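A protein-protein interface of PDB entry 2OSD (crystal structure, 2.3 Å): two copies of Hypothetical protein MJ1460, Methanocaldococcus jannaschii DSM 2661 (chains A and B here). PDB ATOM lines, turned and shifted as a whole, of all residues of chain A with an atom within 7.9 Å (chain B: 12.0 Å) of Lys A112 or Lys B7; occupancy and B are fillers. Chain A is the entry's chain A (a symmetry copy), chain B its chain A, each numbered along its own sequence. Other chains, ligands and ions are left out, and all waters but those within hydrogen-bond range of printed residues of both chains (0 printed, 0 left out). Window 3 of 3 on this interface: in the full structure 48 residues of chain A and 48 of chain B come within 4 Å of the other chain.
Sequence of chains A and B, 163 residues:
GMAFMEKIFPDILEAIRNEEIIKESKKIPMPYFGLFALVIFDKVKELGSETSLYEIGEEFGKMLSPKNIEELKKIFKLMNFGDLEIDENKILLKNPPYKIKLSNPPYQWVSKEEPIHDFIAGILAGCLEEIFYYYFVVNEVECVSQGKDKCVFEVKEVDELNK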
ATOM      1  N   LEU A  53      20.254  28.744  -9.109  1.00  0.00           N
ATOM      2  CA  LEU A  53      21.574  29.317  -8.823  1.00  0.00           C
ATOM      3  C   LEU A  53      22.662  28.902  -9.825  1.00  0.00           C
ATOM      4  O   LEU A  53      23.590  29.664 -10.104  1.00  0.00           O
ATOM      5  CB  LEU A  53      22.034  28.959  -7.404  1.00  0.00           C
ATOM      6  CG  LEU A  53      21.772  29.922  -6.210  1.00  0.00           C
ATOM      7  CD1 LEU A  53      22.313  29.272  -4.909  1.00  0.00           C
ATOM      8  CD2 LEU A  53      22.368  31.319  -6.369  1.00  0.00           C
ATOM      9  N   TYR A 107      32.414  29.186   1.847  1.00  0.00           N
ATOM     10  CA  TYR A 107      31.598  28.298   2.696  1.00  0.00           C
ATOM     11  C   TYR A 107      32.306  27.035   3.174  1.00  0.00           C
ATOM     12  O   TYR A 107      31.690  26.013   3.331  1.00  0.00           O
ATOM     13  CB  TYR A 107      30.303  27.914   1.992  1.00  0.00           C
ATOM     14  CG  TYR A 107      29.508  29.085   1.501  1.00  0.00           C
ATOM     15  CD1 TYR A 107      29.028  30.038   2.392  1.00  0.00           C
ATOM     16  CD2 TYR A 107      29.218  29.235   0.147  1.00  0.00           C
ATOM     17  CE1 TYR A 107      28.303  31.132   1.947  1.00  0.00           C
ATOM     18  CE2 TYR A 107      28.473  30.307  -0.311  1.00  0.00           C
ATOM     19  CZ  TYR A 107      28.009  31.245   0.600  1.00  0.00           C
ATOM     20  OH  TYR A 107      27.272  32.319   0.170  1.00  0.00           O
ATOM     21  N   TRP A 109      33.000  26.487   6.053  1.00  0.00           N
ATOM     22  CA  TRP A 109      32.403  26.210   7.377  1.00  0.00           C
ATOM     23  C   TRP A 109      31.117  25.346   7.290  1.00  0.00           C
ATOM     24  O   TRP A 109      30.686  24.787   8.302  1.00  0.00           O
ATOM     25  CB  TRP A 109      32.160  27.531   8.160  1.00  0.00           C
ATOM     26  CG  TRP A 109      31.563  28.604   7.332  1.00  0.00           C
ATOM     27  CD1 TRP A 109      32.224  29.518   6.563  1.00  0.00           C
ATOM     28  CD2 TRP A 109      30.175  28.833   7.123  1.00  0.00           C
ATOM     29  NE1 TRP A 109      31.317  30.316   5.884  1.00  0.00           N
ATOM     30  CE2 TRP A 109      30.053  29.907   6.217  1.00  0.00           C
ATOM     31  CE3 TRP A 109      29.017  28.217   7.607  1.00  0.00           C
ATOM     32  CZ2 TRP A 109      28.817  30.400   5.800  1.00  0.00           C
ATOM     33  CZ3 TRP A 109      27.793  28.708   7.212  1.00  0.00           C
ATOM     34  CH2 TRP A 109      27.699  29.793   6.323  1.00  0.00           C
ATOM     35  N   VAL A 110      30.527  25.228   6.093  1.00  0.00           N
ATOM     36  CA  VAL A 110      29.304  24.448   5.872  1.00  0.00           C
ATOM     37  C   VAL A 110      29.560  22.972   5.752  1.00  0.00           C
ATOM     38  O   VAL A 110      30.457  22.547   5.074  1.00  0.00           O
ATOM     39  CB  VAL A 110      28.575  24.855   4.604  1.00  0.00           C
ATOM     40  CG1 VAL A 110      27.370  23.933   4.354  1.00  0.00           C
ATOM     41  CG2 VAL A 110      28.147  26.317   4.670  1.00  0.00           C
ATOM     42  N   SER A 111      28.717  22.198   6.421  1.00  0.00           N
ATOM     43  CA  SER A 111      28.795  20.762   6.459  1.00  0.00           C
ATOM     44  C   SER A 111      27.493  20.234   5.852  1.00  0.00           C
ATOM     45  O   SER A 111      26.413  20.532   6.366  1.00  0.00           O
ATOM     46  CB  SER A 111      28.917  20.344   7.924  1.00  0.00           C
ATOM     47  OG  SER A 111      29.767  19.238   8.072  1.00  0.00           O
ATOM     48  N   LYS A 112      27.578  19.475   4.759  1.00  0.00           N
ATOM     49  CA  LYS A 112      26.377  18.965   4.084  1.00  0.00           C
ATOM     50  C   LYS A 112      26.687  17.675   3.315  1.00  0.00           C
ATOM     51  O   LYS A 112      27.791  17.523   2.808  1.00  0.00           O
ATOM     52  CB  LYS A 112      25.839  20.044   3.140  1.00  0.00           C
ATOM     53  CG  LYS A 112      24.362  20.398   3.325  1.00  0.00           C
ATOM     54  CD  LYS A 112      24.064  21.897   3.022  1.00  0.00           C
ATOM     55  CE  LYS A 112      22.998  22.457   3.990  1.00  0.00           C
ATOM     56  N   GLU A 113      25.720  16.758   3.250  1.00  0.00           N
ATOM     57  CA  GLU A 113      25.832  15.499   2.489  1.00  0.00           C
ATOM     58  C   GLU A 113      26.082  15.729   1.002  1.00  0.00           C
ATOM     59  O   GLU A 113      26.982  15.105   0.415  1.00  0.00           O
ATOM     60  CB  GLU A 113      24.551  14.648   2.674  1.00  0.00           C
ATOM     61  CG  GLU A 113      24.540  13.256   2.008  1.00  0.00           C
ATOM     62  CD  GLU A 113      23.371  12.372   2.496  1.00  0.00           C
ATOM     63  N   GLU A 114      25.292  16.617   0.385  1.00  0.00           N
ATOM     64  CA  GLU A 114      25.467  16.887  -1.041  1.00  0.00           C
ATOM     65  C   GLU A 114      26.264  18.183  -1.268  1.00  0.00           C
ATOM     66  O   GLU A 114      26.252  19.078  -0.425  1.00  0.00           O
ATOM     67  CB  GLU A 114      24.121  16.880  -1.784  1.00  0.00           C
ATOM     68  CG  GLU A 114      23.473  15.453  -1.919  1.00  0.00           C
ATOM     69  CD  GLU A 114      24.288  14.444  -2.770  1.00  0.00           C
ATOM     70  N   PRO A 115      27.006  18.263  -2.392  1.00  0.00           N
ATOM     71  CA  PRO A 115      27.785  19.441  -2.723  1.00  0.00           C
ATOM     72  C   PRO A 115      26.945  20.710  -2.733  1.00  0.00           C
ATOM     73  O   PRO A 115      25.778  20.661  -3.109  1.00  0.00           O
ATOM     74  CB  PRO A 115      28.298  19.122  -4.115  1.00  0.00           C
ATOM     75  CG  PRO A 115      28.335  17.657  -4.171  1.00  0.00           C
ATOM     76  CD  PRO A 115      27.179  17.201  -3.403  1.00  0.00           C
ATOM     77  N   ILE A 116      27.550  21.828  -2.325  1.00  0.00           N
ATOM     78  CA  ILE A 116      26.850  23.080  -2.143  1.00  0.00           C
ATOM     79  C   ILE A 116      27.212  24.142  -3.163  1.00  0.00           C
ATOM     80  O   ILE A 116      26.519  25.140  -3.245  1.00  0.00           O
ATOM     81  CB  ILE A 116      27.082  23.682  -0.720  1.00  0.00           C
ATOM     82  CG1 ILE A 116      28.547  24.083  -0.483  1.00  0.00           C
ATOM     83  CG2 ILE A 116      26.588  22.714   0.368  1.00  0.00           C
ATOM     84  CD1 ILE A 116      28.790  24.914   0.806  1.00  0.00           C
ATOM     85  N   ASP A 118      26.748  25.148  -6.288  1.00  0.00           N
ATOM     86  CA  ASP A 118      26.016  25.205  -7.535  1.00  0.00           C
ATOM     87  C   ASP A 118      26.290  26.475  -8.312  1.00  0.00           C
ATOM     88  O   ASP A 118      26.420  26.459  -9.533  1.00  0.00           O
ATOM     89  CB  ASP A 118      24.521  25.136  -7.272  1.00  0.00           C
ATOM     90  CG  ASP A 118      24.071  23.781  -6.837  1.00  0.00           C
ATOM     91  OD1 ASP A 118      24.937  22.948  -6.467  1.00  0.00           O
ATOM     92  OD2 ASP A 118      22.841  23.568  -6.843  1.00  0.00           O
ATOM     93  N   CYS A 143      32.732  17.838  -2.776  1.00  0.00           N
ATOM     94  CA  CYS A 143      32.673  19.153  -2.171  1.00  0.00           C
ATOM     95  C   CYS A 143      33.371  19.158  -0.830  1.00  0.00           C
ATOM     96  O   CYS A 143      33.292  18.207  -0.083  1.00  0.00           O
ATOM     97  CB  CYS A 143      31.221  19.572  -1.997  1.00  0.00           C
ATOM     98  SG  CYS A 143      30.904  21.315  -1.573  1.00  0.00           S
ATOM     99  N   VAL A 144      34.092  20.227  -0.554  1.00  0.00           N
ATOM    100  CA  VAL A 144      34.588  20.527   0.805  1.00  0.00           C
ATOM    101  C   VAL A 144      33.481  20.382   1.893  1.00  0.00           C
ATOM    102  O   VAL A 144      33.759  19.966   3.003  1.00  0.00           O
ATOM    103  CB  VAL A 144      35.295  21.936   0.808  1.00  0.00           C
ATOM    104  CG1 VAL A 144      35.592  22.403   2.180  1.00  0.00           C
ATOM    105  CG2 VAL A 144      36.599  21.840   0.039  1.00  0.00           C
ATOM    106  N   SER A 145      32.228  20.657   1.533  1.00  0.00           N
ATOM    107  CA  SER A 145      31.059  20.448   2.410  1.00  0.00           C
ATOM    108  C   SER A 145      30.931  19.031   2.961  1.00  0.00           C
ATOM    109  O   SER A 145      30.267  18.812   3.981  1.00  0.00           O
ATOM    110  CB  SER A 145      29.731  20.841   1.692  1.00  0.00           C
ATOM    111  OG  SER A 145      29.108  19.739   1.002  1.00  0.00           O
ATOM    112  N   GLN A 146      31.549  18.066   2.284  1.00  0.00           N
ATOM    113  CA  GLN A 146      31.495  16.675   2.687  1.00  0.00           C
ATOM    114  C   GLN A 146      32.751  16.237   3.426  1.00  0.00           C
ATOM    115  O   GLN A 146      32.930  15.044   3.685  1.00  0.00           O
ATOM    116  CB  GLN A 146      31.324  15.808   1.448  1.00  0.00           C
ATOM    117  CG  GLN A 146      30.174  16.230   0.576  1.00  0.00           C
ATOM    118  CD  GLN A 146      30.207  15.611  -0.803  1.00  0.00           C
ATOM    119  OE1 GLN A 146      31.305  15.443  -1.390  1.00  0.00           O
ATOM    120  NE2 GLN A 146      28.991  15.283  -1.338  1.00  0.00           N
ATOM    121  N   GLY A 147      33.621  17.182   3.764  1.00  0.00           N
ATOM    122  CA  GLY A 147      34.867  16.860   4.452  1.00  0.00           C
ATOM    123  C   GLY A 147      36.021  16.533   3.521  1.00  0.00           C
ATOM    124  O   GLY A 147      37.061  16.030   3.957  1.00  0.00           O
ATOM    125  N   GLU B   6      17.545  26.951  -2.402  1.00  0.00           N
ATOM    126  CA  GLU B   6      18.866  26.260  -2.485  1.00  0.00           C
ATOM    127  C   GLU B   6      19.180  25.516  -1.176  1.00  0.00           C
ATOM    128  O   GLU B   6      18.590  25.809  -0.128  1.00  0.00           O
ATOM    129  CB  GLU B   6      19.972  27.265  -2.831  1.00  0.00           C
ATOM    130  N   LYS B   7      20.094  24.544  -1.254  1.00  0.00           N
ATOM    131  CA  LYS B   7      20.512  23.736  -0.091  1.00  0.00           C
ATOM    132  C   LYS B   7      21.366  24.542   0.916  1.00  0.00           C
ATOM    133  O   LYS B   7      21.333  24.263   2.120  1.00  0.00           O
ATOM    134  CB  LYS B   7      21.270  22.474  -0.550  1.00  0.00           C
ATOM    135  N   ILE B   8      22.098  25.545   0.413  1.00  0.00           N
ATOM    136  CA  ILE B   8      22.995  26.396   1.222  1.00  0.00           C
ATOM    137  C   ILE B   8      22.268  27.440   2.098  1.00  0.00           C
ATOM    138  O   ILE B   8      22.856  27.992   3.024  1.00  0.00           O
ATOM    139  CB  ILE B   8      23.996  27.156   0.295  1.00  0.00           C
ATOM    140  CG1 ILE B   8      25.264  27.569   1.049  1.00  0.00           C
ATOM    141  CG2 ILE B   8      23.333  28.386  -0.359  1.00  0.00           C
ATOM    142  CD1 ILE B   8      26.352  28.013   0.128  1.00  0.00           C
ATOM    143  N   PHE B   9      20.997  27.702   1.803  1.00  0.00           N
ATOM    144  CA  PHE B   9      20.221  28.756   2.482  1.00  0.00           C
ATOM    145  C   PHE B   9      20.011  28.605   4.012  1.00  0.00           C
ATOM    146  O   PHE B   9      20.134  29.576   4.735  1.00  0.00           O
ATOM    147  CB  PHE B   9      18.886  28.992   1.742  1.00  0.00           C
ATOM    148  CG  PHE B   9      19.035  29.684   0.391  1.00  0.00           C
ATOM    149  CD1 PHE B   9      20.241  30.275  -0.012  1.00  0.00           C
ATOM    150  CD2 PHE B   9      17.949  29.785  -0.463  1.00  0.00           C
ATOM    151  CE1 PHE B   9      20.362  30.928  -1.250  1.00  0.00           C
ATOM    152  CE2 PHE B   9      18.062  30.440  -1.702  1.00  0.00           C
ATOM    153  CZ  PHE B   9      19.273  31.011  -2.090  1.00  0.00           C
ATOM    154  N   PRO B  10      19.683  27.407   4.508  1.00  0.00           N
ATOM    155  CA  PRO B  10      19.733  27.197   5.980  1.00  0.00           C
ATOM    156  C   PRO B  10      21.028  27.670   6.694  1.00  0.00           C
ATOM    157  O   PRO B  10      20.977  28.339   7.718  1.00  0.00           O
ATOM    158  CB  PRO B  10      19.571  25.672   6.130  1.00  0.00           C
ATOM    159  CG  PRO B  10      19.445  25.103   4.748  1.00  0.00           C
ATOM    160  CD  PRO B  10      19.184  26.223   3.790  1.00  0.00           C
ATOM    161  N   ASP B  11      22.172  27.301   6.133  1.00  0.00           N
ATOM    162  CA  ASP B  11      23.479  27.663   6.665  1.00  0.00           C
ATOM    163  C   ASP B  11      23.750  29.158   6.664  1.00  0.00           C
ATOM    164  O   ASP B  11      24.581  29.628   7.410  1.00  0.00           O
ATOM    165  CB  ASP B  11      24.569  26.998   5.829  1.00  0.00           C
ATOM    166  CG  ASP B  11      24.522  25.499   5.900  1.00  0.00           C
ATOM    167  OD1 ASP B  11      24.961  24.926   6.930  1.00  0.00           O
ATOM    168  OD2 ASP B  11      24.056  24.906   4.907  1.00  0.00           O
ATOM    169  N   ILE B  12      23.082  29.893   5.790  1.00  0.00           N
ATOM    170  CA  ILE B  12      23.274  31.335   5.684  1.00  0.00           C
ATOM    171  C   ILE B  12      22.606  32.112   6.817  1.00  0.00           C
ATOM    172  O   ILE B  12      23.142  33.104   7.283  1.00  0.00           O
ATOM    173  CB  ILE B  12      22.810  31.859   4.297  1.00  0.00           C
ATOM    174  CG1 ILE B  12      23.979  31.756   3.292  1.00  0.00           C
ATOM    175  CG2 ILE B  12      22.363  33.296   4.391  1.00  0.00           C
ATOM    176  CD1 ILE B  12      23.574  31.524   1.839  1.00  0.00           C
ATOM    177  N   LEU B  13      21.442  31.671   7.266  1.00  0.00           N
ATOM    178  CA  LEU B  13      20.780  32.351   8.347  1.00  0.00           C
ATOM    179  C   LEU B  13      21.538  32.163   9.659  1.00  0.00           C
ATOM    180  O   LEU B  13      21.604  33.094  10.462  1.00  0.00           O
ATOM    181  CB  LEU B  13      19.327  31.889   8.476  1.00  0.00           C
ATOM    182  CG  LEU B  13      18.397  32.461   7.397  1.00  0.00           C
ATOM    183  CD1 LEU B  13      17.052  31.714   7.373  1.00  0.00           C
ATOM    184  CD2 LEU B  13      18.221  33.974   7.589  1.00  0.00           C
ATOM    185  N   GLU B  14      22.112  30.981   9.873  1.00  0.00           N
ATOM    186  CA  GLU B  14      22.961  30.731  11.043  1.00  0.00           C
ATOM    187  C   GLU B  14      24.242  31.527  10.984  1.00  0.00           C
ATOM    188  O   GLU B  14      24.701  32.037  11.990  1.00  0.00           O
ATOM    189  CB  GLU B  14      23.287  29.244  11.152  1.00  0.00           C
ATOM    190  CG  GLU B  14      22.054  28.393  11.459  1.00  0.00           C
ATOM    191  CD  GLU B  14      22.359  26.903  11.753  1.00  0.00           C
ATOM    192  OE1 GLU B  14      23.228  26.292  11.071  1.00  0.00           O
ATOM    193  OE2 GLU B  14      21.693  26.340  12.663  1.00  0.00           O
ATOM    194  N   ALA B  15      24.812  31.650   9.788  1.00  0.00           N
ATOM    195  CA  ALA B  15      26.060  32.347   9.587  1.00  0.00           C
ATOM    196  C   ALA B  15      25.956  33.799   9.983  1.00  0.00           C
ATOM    197  O   ALA B  15      26.864  34.343  10.598  1.00  0.00           O
ATOM    198  CB  ALA B  15      26.480  32.250   8.130  1.00  0.00           C
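No position is printed for both chains.
Lys A112 touches just these residues of chain B: Lys B7 and Asp B11. Lys B7 touches just one residue of chain A: Lys A112 (3.1 Å). Ser A111 touches none of the printed residues of chain B. No residue of chain B comes within 4 Å of Pro A115. No residue of chain B comes within 4 Å of Ser A145. No residue of chain B comes within 4 Å of Gln A146. Printed residues of chain A within 4 Å of Ala B15: Trp A109. Of the printed residues of chain B, Trp A109 touches Asp B11 and Ala B15. Ile A116 touches none of the printed residues of chain B. The nearest residue of chain B that does not touch Lys A112 is Pro B10 (4.5 Å). The nearest printed residue of chain A that does not touch Asp B11 is Ser A111 (4.7 Å).
Of the 10 printed residues of chain B, 5 touch a printed residue of chain A. Of the 16 printed residues of chain A, 5 touch a printed residue of chain B. Printed residues of chain A that touch a printed residue of chain B: Leu A53, Tyr A107, Trp A109, Val A110 and Lys A112. Hydrophobic or aromatic side chains of chain A within 4 Å of the printed part of chain B: Leu A53, Tyr A107, Trp A109 and Val A110. Among the printed residues, 7 pairs touch across the chains.
O of Ser A145 is in hydrogen-bond range of N of Lys A112, at 2.9 Å.
CD1 of Leu A53 touches CB of Glu B6, 3.7 Å away. CD2 of Tyr A107 touches CD1 of Ile B8, 3.1 Å away. CH2 of Trp A109 touches O of Asp B11, 3.3 Å away. Trp A109 touches Ala B15 (CH2 to CB, 3.3 Å). Asp B11 touches Val A110. Lys B7 touches Lys A112 (O to CE, 3.1 Å). Lys A112 touches Asp B11 (CE to OD2, 2.8 Å).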
